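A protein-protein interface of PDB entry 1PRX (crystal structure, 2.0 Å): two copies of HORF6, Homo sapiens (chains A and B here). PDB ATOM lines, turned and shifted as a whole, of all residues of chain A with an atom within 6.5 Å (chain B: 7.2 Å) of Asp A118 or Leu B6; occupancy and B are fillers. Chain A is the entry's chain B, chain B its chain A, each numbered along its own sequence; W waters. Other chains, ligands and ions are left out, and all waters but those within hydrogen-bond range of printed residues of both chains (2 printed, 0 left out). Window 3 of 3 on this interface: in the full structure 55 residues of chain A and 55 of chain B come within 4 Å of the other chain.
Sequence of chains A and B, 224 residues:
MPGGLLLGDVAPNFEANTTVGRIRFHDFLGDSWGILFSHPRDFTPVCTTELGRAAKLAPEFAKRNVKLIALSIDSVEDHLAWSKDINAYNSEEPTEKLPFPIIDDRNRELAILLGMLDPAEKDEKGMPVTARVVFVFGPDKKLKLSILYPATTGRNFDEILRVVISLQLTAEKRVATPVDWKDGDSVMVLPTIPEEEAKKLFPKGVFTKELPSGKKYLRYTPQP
The backbone carbonyl oxygen of Ser B146 lies within hydrogen-bond range of the backbone NH of Leu A148 (2.9 Å).
The backbone NH (N) of Leu B6 lies within hydrogen-bond range of the side-chain carboxylate (OD2) of Asp B9, 2.8 Å away. The backbone carbonyl oxygen (O) of Ala A111 is in hydrogen-bond range of the backbone NH (N) of Met A116. OG1 of Thr A130 lies within hydrogen-bond range of O of Met A116, at 3.0 Å. N of Ala A120 lies within hydrogen-bond range of OD1 of Asp A118, 2.8 Å away.
Pro A2 touches Leu B5 (O to O, 3.7 Å). OG of Ser B146 touches CG of Pro A2, 3.8 Å away. CD2 of Leu B6 touches O of Gly A115, at 3.3 Å. Met A116 touches Leu B6 (CA to CD2, 3.9 Å). Leu B6 touches Asp A118. Thr A130 touches Leu B6 (CG2 to CB, 3.9 Å). Thr A130 touches Leu B7. Leu A148 touches Leu B7 (CD2 to CD1, 3.5 Å). Leu A148 touches Leu B145.
Of the printed residues of chain B, Asp A118 touches Leu B6. Of the printed residues of chain A, Leu B6 touches Gly A115 (3.3 Å), Met A116 (3.9 Å), Asp A118 (3.998 Å) and Thr A130 (3.9 Å). Printed residues of chain A within 4 Å of Leu B145: Leu A148 (3.5 Å). Printed residues of chain B within 4 Å of Pro A2: Leu B5 and Ser B146. Of the printed residues of chain A, Ser B146 touches Pro A2 and Leu A148. Of the printed residues of chain B, Leu A148 touches Leu B7, Leu B145 and Ser B146. The nearest printed residue of chain B that does not touch Asp A118 is Asp B9 (6.0 Å). The nearest printed residue of chain A that does not touch Leu B6 is Leu A117 (4.1 Å).
Of the 14 printed residues of chain A, 6 touch a printed residue of chain B. Printed residues of chain A that touch a printed residue of chain B: Pro A2, Gly A115, Met A116, Asp A118, Thr A130 and Leu A148. Of the 11 printed residues of chain B, 5 touch a printed residue of chain A. Hydrophobic or aromatic side chains of chain B that line the printed part of chain A: Leu B6, Leu B7 and Leu B145. Among the printed residues, 10 pairs touch across the chains.
No position is printed for both chains.
Water W2 bridges the side-chain carboxylate of Asp B9 (2.7 Å) and the side-chain carboxylate of Glu A121 (2.9 Å). Water W1 bridges the backbone NH of Leu B7 (3.1 Å) and the backbone carbonyl oxygen of Thr A130 (3.1 Å).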
ATOM      1  N   PRO A   2      28.707  17.053  23.694  1.00  0.00           N
ATOM      2  CA  PRO A   2      29.042  17.927  24.840  1.00  0.00           C
ATOM      3  C   PRO A   2      27.838  17.914  25.785  1.00  0.00           C
ATOM      4  O   PRO A   2      27.300  16.835  26.066  1.00  0.00           O
ATOM      5  CB  PRO A   2      29.268  19.325  24.275  1.00  0.00           C
ATOM      6  CG  PRO A   2      29.677  19.008  22.822  1.00  0.00           C
ATOM      7  CD  PRO A   2      28.760  17.813  22.439  1.00  0.00           C
ATOM      8  N   GLY A   3      27.401  19.090  26.253  1.00  0.00           N
ATOM      9  CA  GLY A   3      26.240  19.177  27.121  1.00  0.00           C
ATOM     10  C   GLY A   3      24.982  18.996  26.296  1.00  0.00           C
ATOM     11  O   GLY A   3      25.065  18.706  25.099  1.00  0.00           O
ATOM     12  N   GLY A   4      23.820  19.174  26.917  1.00  0.00           N
ATOM     13  CA  GLY A   4      22.574  19.011  26.183  1.00  0.00           C
ATOM     14  C   GLY A   4      22.170  20.234  25.382  1.00  0.00           C
ATOM     15  O   GLY A   4      21.166  20.208  24.676  1.00  0.00           O
ATOM     16  N   ALA A 111      22.546  18.675  36.877  1.00  0.00           N
ATOM     17  CA  ALA A 111      23.354  17.877  35.962  1.00  0.00           C
ATOM     18  C   ALA A 111      22.462  17.247  34.897  1.00  0.00           C
ATOM     19  O   ALA A 111      22.896  17.001  33.771  1.00  0.00           O
ATOM     20  CB  ALA A 111      24.105  16.790  36.739  1.00  0.00           C
ATOM     21  N   ILE A 112      21.218  16.970  35.270  1.00  0.00           N
ATOM     22  CA  ILE A 112      20.240  16.390  34.356  1.00  0.00           C
ATOM     23  C   ILE A 112      19.689  17.492  33.454  1.00  0.00           C
ATOM     24  O   ILE A 112      19.570  17.312  32.238  1.00  0.00           O
ATOM     25  CB  ILE A 112      19.085  15.705  35.134  1.00  0.00           C
ATOM     26  CG1 ILE A 112      19.637  14.540  35.962  1.00  0.00           C
ATOM     27  CG2 ILE A 112      18.005  15.198  34.178  1.00  0.00           C
ATOM     28  CD1 ILE A 112      18.587  13.801  36.766  1.00  0.00           C
ATOM     29  N   GLY A 115      21.988  18.505  30.769  1.00  0.00           N
ATOM     30  CA  GLY A 115      22.288  17.381  29.903  1.00  0.00           C
ATOM     31  C   GLY A 115      23.634  16.694  30.007  1.00  0.00           C
ATOM     32  O   GLY A 115      24.185  16.290  28.982  1.00  0.00           O
ATOM     33  N   MET A 116      24.172  16.548  31.213  1.00  0.00           N
ATOM     34  CA  MET A 116      25.456  15.870  31.363  1.00  0.00           C
ATOM     35  C   MET A 116      25.377  14.702  32.338  1.00  0.00           C
ATOM     36  O   MET A 116      26.339  14.391  33.035  1.00  0.00           O
ATOM     37  CB  MET A 116      26.551  16.853  31.767  1.00  0.00           C
ATOM     38  CG  MET A 116      26.278  17.632  33.021  1.00  0.00           C
ATOM     39  SD  MET A 116      27.465  18.959  33.221  1.00  0.00           S
ATOM     40  CE  MET A 116      26.825  19.697  34.728  1.00  0.00           C
ATOM     41  N   LEU A 117      24.220  14.051  32.368  1.00  0.00           N
ATOM     42  CA  LEU A 117      24.004  12.922  33.251  1.00  0.00           C
ATOM     43  C   LEU A 117      22.837  12.075  32.757  1.00  0.00           C
ATOM     44  O   LEU A 117      21.802  12.616  32.338  1.00  0.00           O
ATOM     45  CB  LEU A 117      23.722  13.422  34.667  1.00  0.00           C
ATOM     46  CG  LEU A 117      23.749  12.344  35.744  1.00  0.00           C
ATOM     47  CD1 LEU A 117      24.478  12.862  36.955  1.00  0.00           C
ATOM     48  CD2 LEU A 117      22.344  11.872  36.081  1.00  0.00           C
ATOM     49  N   ASP A 118      23.025  10.753  32.798  1.00  0.00           N
ATOM     50  CA  ASP A 118      22.016   9.778  32.384  1.00  0.00           C
ATOM     51  C   ASP A 118      21.514   9.043  33.631  1.00  0.00           C
ATOM     52  O   ASP A 118      22.259   8.285  34.257  1.00  0.00           O
ATOM     53  CB  ASP A 118      22.628   8.772  31.401  1.00  0.00           C
ATOM     54  CG  ASP A 118      21.606   7.791  30.835  1.00  0.00           C
ATOM     55  OD1 ASP A 118      20.507   7.630  31.417  1.00  0.00           O
ATOM     56  OD2 ASP A 118      21.888   7.181  29.778  1.00  0.00           O
ATOM     57  N   PRO A 119      20.238   9.256  34.008  1.00  0.00           N
ATOM     58  CA  PRO A 119      19.641   8.609  35.188  1.00  0.00           C
ATOM     59  C   PRO A 119      19.614   7.080  35.093  1.00  0.00           C
ATOM     60  O   PRO A 119      19.592   6.389  36.110  1.00  0.00           O
ATOM     61  CB  PRO A 119      18.232   9.197  35.220  1.00  0.00           C
ATOM     62  CG  PRO A 119      18.410  10.560  34.577  1.00  0.00           C
ATOM     63  CD  PRO A 119      19.292  10.215  33.408  1.00  0.00           C
ATOM     64  N   ALA A 120      19.630   6.552  33.870  1.00  0.00           N
ATOM     65  CA  ALA A 120      19.627   5.105  33.661  1.00  0.00           C
ATOM     66  C   ALA A 120      21.016   4.501  33.883  1.00  0.00           C
ATOM     67  O   ALA A 120      21.219   3.312  33.629  1.00  0.00           O
ATOM     68  CB  ALA A 120      19.114   4.758  32.257  1.00  0.00           C
ATOM     69  N   GLU A 121      21.964   5.322  34.338  1.00  0.00           N
ATOM     70  CA  GLU A 121      23.332   4.878  34.620  1.00  0.00           C
ATOM     71  C   GLU A 121      23.618   4.835  36.126  1.00  0.00           C
ATOM     72  O   GLU A 121      24.291   3.870  36.562  1.00  0.00           O
ATOM     73  CB  GLU A 121      24.344   5.804  33.958  1.00  0.00           C
ATOM     74  CG  GLU A 121      25.301   5.097  33.022  1.00  0.00           C
ATOM     75  CD  GLU A 121      25.017   5.411  31.572  1.00  0.00           C
ATOM     76  OE1 GLU A 121      24.129   4.755  30.979  1.00  0.00           O
ATOM     77  OE2 GLU A 121      25.680   6.321  31.033  1.00  0.00           O
ATOM     78  N   THR A 130      30.295  11.762  33.973  1.00  0.00           N
ATOM     79  CA  THR A 130      29.826  12.559  32.835  1.00  0.00           C
ATOM     80  C   THR A 130      29.651  14.061  33.133  1.00  0.00           C
ATOM     81  O   THR A 130      29.662  14.885  32.224  1.00  0.00           O
ATOM     82  CB  THR A 130      28.495  11.997  32.301  1.00  0.00           C
ATOM     83  OG1 THR A 130      27.630  11.698  33.410  1.00  0.00           O
ATOM     84  CG2 THR A 130      28.735  10.734  31.489  1.00  0.00           C
ATOM     85  N   LEU A 148      34.473  19.477  26.917  1.00  0.00           N
ATOM     86  CA  LEU A 148      34.156  18.260  27.677  1.00  0.00           C
ATOM     87  C   LEU A 148      35.364  17.348  27.866  1.00  0.00           C
ATOM     88  O   LEU A 148      35.575  16.412  27.093  1.00  0.00           O
ATOM     89  CB  LEU A 148      33.012  17.458  27.016  1.00  0.00           C
ATOM     90  CG  LEU A 148      31.939  16.720  27.859  1.00  0.00           C
ATOM     91  CD1 LEU A 148      31.352  15.575  27.078  1.00  0.00           C
ATOM     92  CD2 LEU A 148      32.482  16.219  29.152  1.00  0.00           C
ATOM     93  N   LEU B   5      26.319  13.126  22.473  1.00  0.00           N
ATOM     94  CA  LEU B   5      26.768  11.909  23.214  1.00  0.00           C
ATOM     95  C   LEU B   5      27.405  12.379  24.513  1.00  0.00           C
ATOM     96  O   LEU B   5      27.890  13.512  24.593  1.00  0.00           O
ATOM     97  CB  LEU B   5      27.834  11.122  22.422  1.00  0.00           C
ATOM     98  CG  LEU B   5      27.831  10.890  20.908  1.00  0.00           C
ATOM     99  CD1 LEU B   5      29.025  10.015  20.564  1.00  0.00           C
ATOM    100  CD2 LEU B   5      26.565  10.236  20.436  1.00  0.00           C
ATOM    101  N   LEU B   6      27.340  11.545  25.541  1.00  0.00           N
ATOM    102  CA  LEU B   6      27.954  11.855  26.815  1.00  0.00           C
ATOM    103  C   LEU B   6      29.281  11.095  26.814  1.00  0.00           C
ATOM    104  O   LEU B   6      29.563  10.308  25.898  1.00  0.00           O
ATOM    105  CB  LEU B   6      27.078  11.357  27.968  1.00  0.00           C
ATOM    106  CG  LEU B   6      25.669  11.931  28.141  1.00  0.00           C
ATOM    107  CD1 LEU B   6      24.984  11.264  29.346  1.00  0.00           C
ATOM    108  CD2 LEU B   6      25.729  13.444  28.325  1.00  0.00           C
ATOM    109  N   LEU B   7      30.132  11.375  27.793  1.00  0.00           N
ATOM    110  CA  LEU B   7      31.399  10.661  27.876  1.00  0.00           C
ATOM    111  C   LEU B   7      31.063   9.184  28.105  1.00  0.00           C
ATOM    112  O   LEU B   7      30.210   8.871  28.940  1.00  0.00           O
ATOM    113  CB  LEU B   7      32.240  11.194  29.032  1.00  0.00           C
ATOM    114  CG  LEU B   7      32.797  12.606  28.854  1.00  0.00           C
ATOM    115  CD1 LEU B   7      33.558  13.028  30.103  1.00  0.00           C
ATOM    116  CD2 LEU B   7      33.700  12.632  27.647  1.00  0.00           C
ATOM    117  N   GLY B   8      31.706   8.288  27.357  1.00  0.00           N
ATOM    118  CA  GLY B   8      31.436   6.870  27.514  1.00  0.00           C
ATOM    119  C   GLY B   8      30.438   6.316  26.518  1.00  0.00           C
ATOM    120  O   GLY B   8      30.317   5.089  26.374  1.00  0.00           O
ATOM    121  N   ASP B   9      29.736   7.200  25.812  1.00  0.00           N
ATOM    122  CA  ASP B   9      28.748   6.789  24.810  1.00  0.00           C
ATOM    123  C   ASP B   9      29.459   6.169  23.639  1.00  0.00           C
ATOM    124  O   ASP B   9      30.490   6.675  23.199  1.00  0.00           O
ATOM    125  CB  ASP B   9      27.944   7.990  24.296  1.00  0.00           C
ATOM    126  CG  ASP B   9      26.800   8.381  25.218  1.00  0.00           C
ATOM    127  OD1 ASP B   9      26.720   7.860  26.336  1.00  0.00           O
ATOM    128  OD2 ASP B   9      25.986   9.251  24.824  1.00  0.00           O
ATOM    129  N   VAL B  10      28.887   5.094  23.118  1.00  0.00           N
ATOM    130  CA  VAL B  10      29.454   4.401  21.970  1.00  0.00           C
ATOM    131  C   VAL B  10      29.091   5.159  20.706  1.00  0.00           C
ATOM    132  O   VAL B  10      27.947   5.578  20.542  1.00  0.00           O
ATOM    133  CB  VAL B  10      28.905   2.959  21.855  1.00  0.00           C
ATOM    134  CG1 VAL B  10      29.515   2.250  20.648  1.00  0.00           C
ATOM    135  CG2 VAL B  10      29.212   2.186  23.121  1.00  0.00           C
ATOM    136  N   LYS B 142      34.158   4.317  22.241  1.00  0.00           N
ATOM    137  CA  LYS B 142      33.521   5.188  23.236  1.00  0.00           C
ATOM    138  C   LYS B 142      34.077   6.618  23.262  1.00  0.00           C
ATOM    139  O   LYS B 142      35.276   6.830  23.071  1.00  0.00           O
ATOM    140  CB  LYS B 142      33.626   4.564  24.630  1.00  0.00           C
ATOM    141  CG  LYS B 142      32.776   3.326  24.798  1.00  0.00           C
ATOM    142  CD  LYS B 142      33.042   2.630  26.122  1.00  0.00           C
ATOM    143  CE  LYS B 142      32.080   1.471  26.304  1.00  0.00           C
ATOM    144  NZ  LYS B 142      32.090   0.512  25.141  1.00  0.00           N
ATOM    145  N   LEU B 143      33.196   7.581  23.528  1.00  0.00           N
ATOM    146  CA  LEU B 143      33.569   8.988  23.583  1.00  0.00           C
ATOM    147  C   LEU B 143      34.489   9.217  24.772  1.00  0.00           C
ATOM    148  O   LEU B 143      34.137   8.900  25.893  1.00  0.00           O
ATOM    149  CB  LEU B 143      32.318   9.854  23.743  1.00  0.00           C
ATOM    150  CG  LEU B 143      32.107  11.159  22.955  1.00  0.00           C
ATOM    151  CD1 LEU B 143      31.664  12.274  23.898  1.00  0.00           C
ATOM    152  CD2 LEU B 143      33.347  11.565  22.190  1.00  0.00           C
ATOM    153  N   LYS B 144      35.669   9.762  24.521  1.00  0.00           N
ATOM    154  CA  LYS B 144      36.616  10.029  25.598  1.00  0.00           C
ATOM    155  C   LYS B 144      36.747  11.525  25.876  1.00  0.00           C
ATOM    156  O   LYS B 144      37.101  11.927  26.977  1.00  0.00           O
ATOM    157  CB  LYS B 144      38.000   9.473  25.236  1.00  0.00           C
ATOM    158  CG  LYS B 144      38.058   7.956  25.072  1.00  0.00           C
ATOM    159  CD  LYS B 144      37.607   7.281  26.356  1.00  0.00           C
ATOM    160  CE  LYS B 144      37.813   5.779  26.324  1.00  0.00           C
ATOM    161  NZ  LYS B 144      37.244   5.223  25.095  1.00  0.00           N
ATOM    162  N   LEU B 145      36.367  12.355  24.908  1.00  0.00           N
ATOM    163  CA  LEU B 145      36.547  13.800  25.052  1.00  0.00           C
ATOM    164  C   LEU B 145      35.902  14.501  23.855  1.00  0.00           C
ATOM    165  O   LEU B 145      35.789  13.914  22.773  1.00  0.00           O
ATOM    166  CB  LEU B 145      38.074  14.033  25.046  1.00  0.00           C
ATOM    167  CG  LEU B 145      39.012  15.242  24.988  1.00  0.00           C
ATOM    168  CD1 LEU B 145      38.466  16.359  24.138  1.00  0.00           C
ATOM    169  CD2 LEU B 145      39.376  15.702  26.363  1.00  0.00           C
ATOM    170  N   SER B 146      35.414  15.721  24.061  1.00  0.00           N
ATOM    171  CA  SER B 146      34.836  16.503  22.972  1.00  0.00           C
ATOM    172  C   SER B 146      35.079  17.988  23.240  1.00  0.00           C
ATOM    173  O   SER B 146      35.276  18.411  24.381  1.00  0.00           O
ATOM    174  CB  SER B 146      33.344  16.190  22.752  1.00  0.00           C
ATOM    175  OG  SER B 146      32.516  16.658  23.799  1.00  0.00           O
HETATM  176  O   HOH W   1      29.194  13.851  29.317  1.00  0.00           O
HETATM  177  O   HOH W   2      26.234   6.015  28.179  1.00  0.00           O
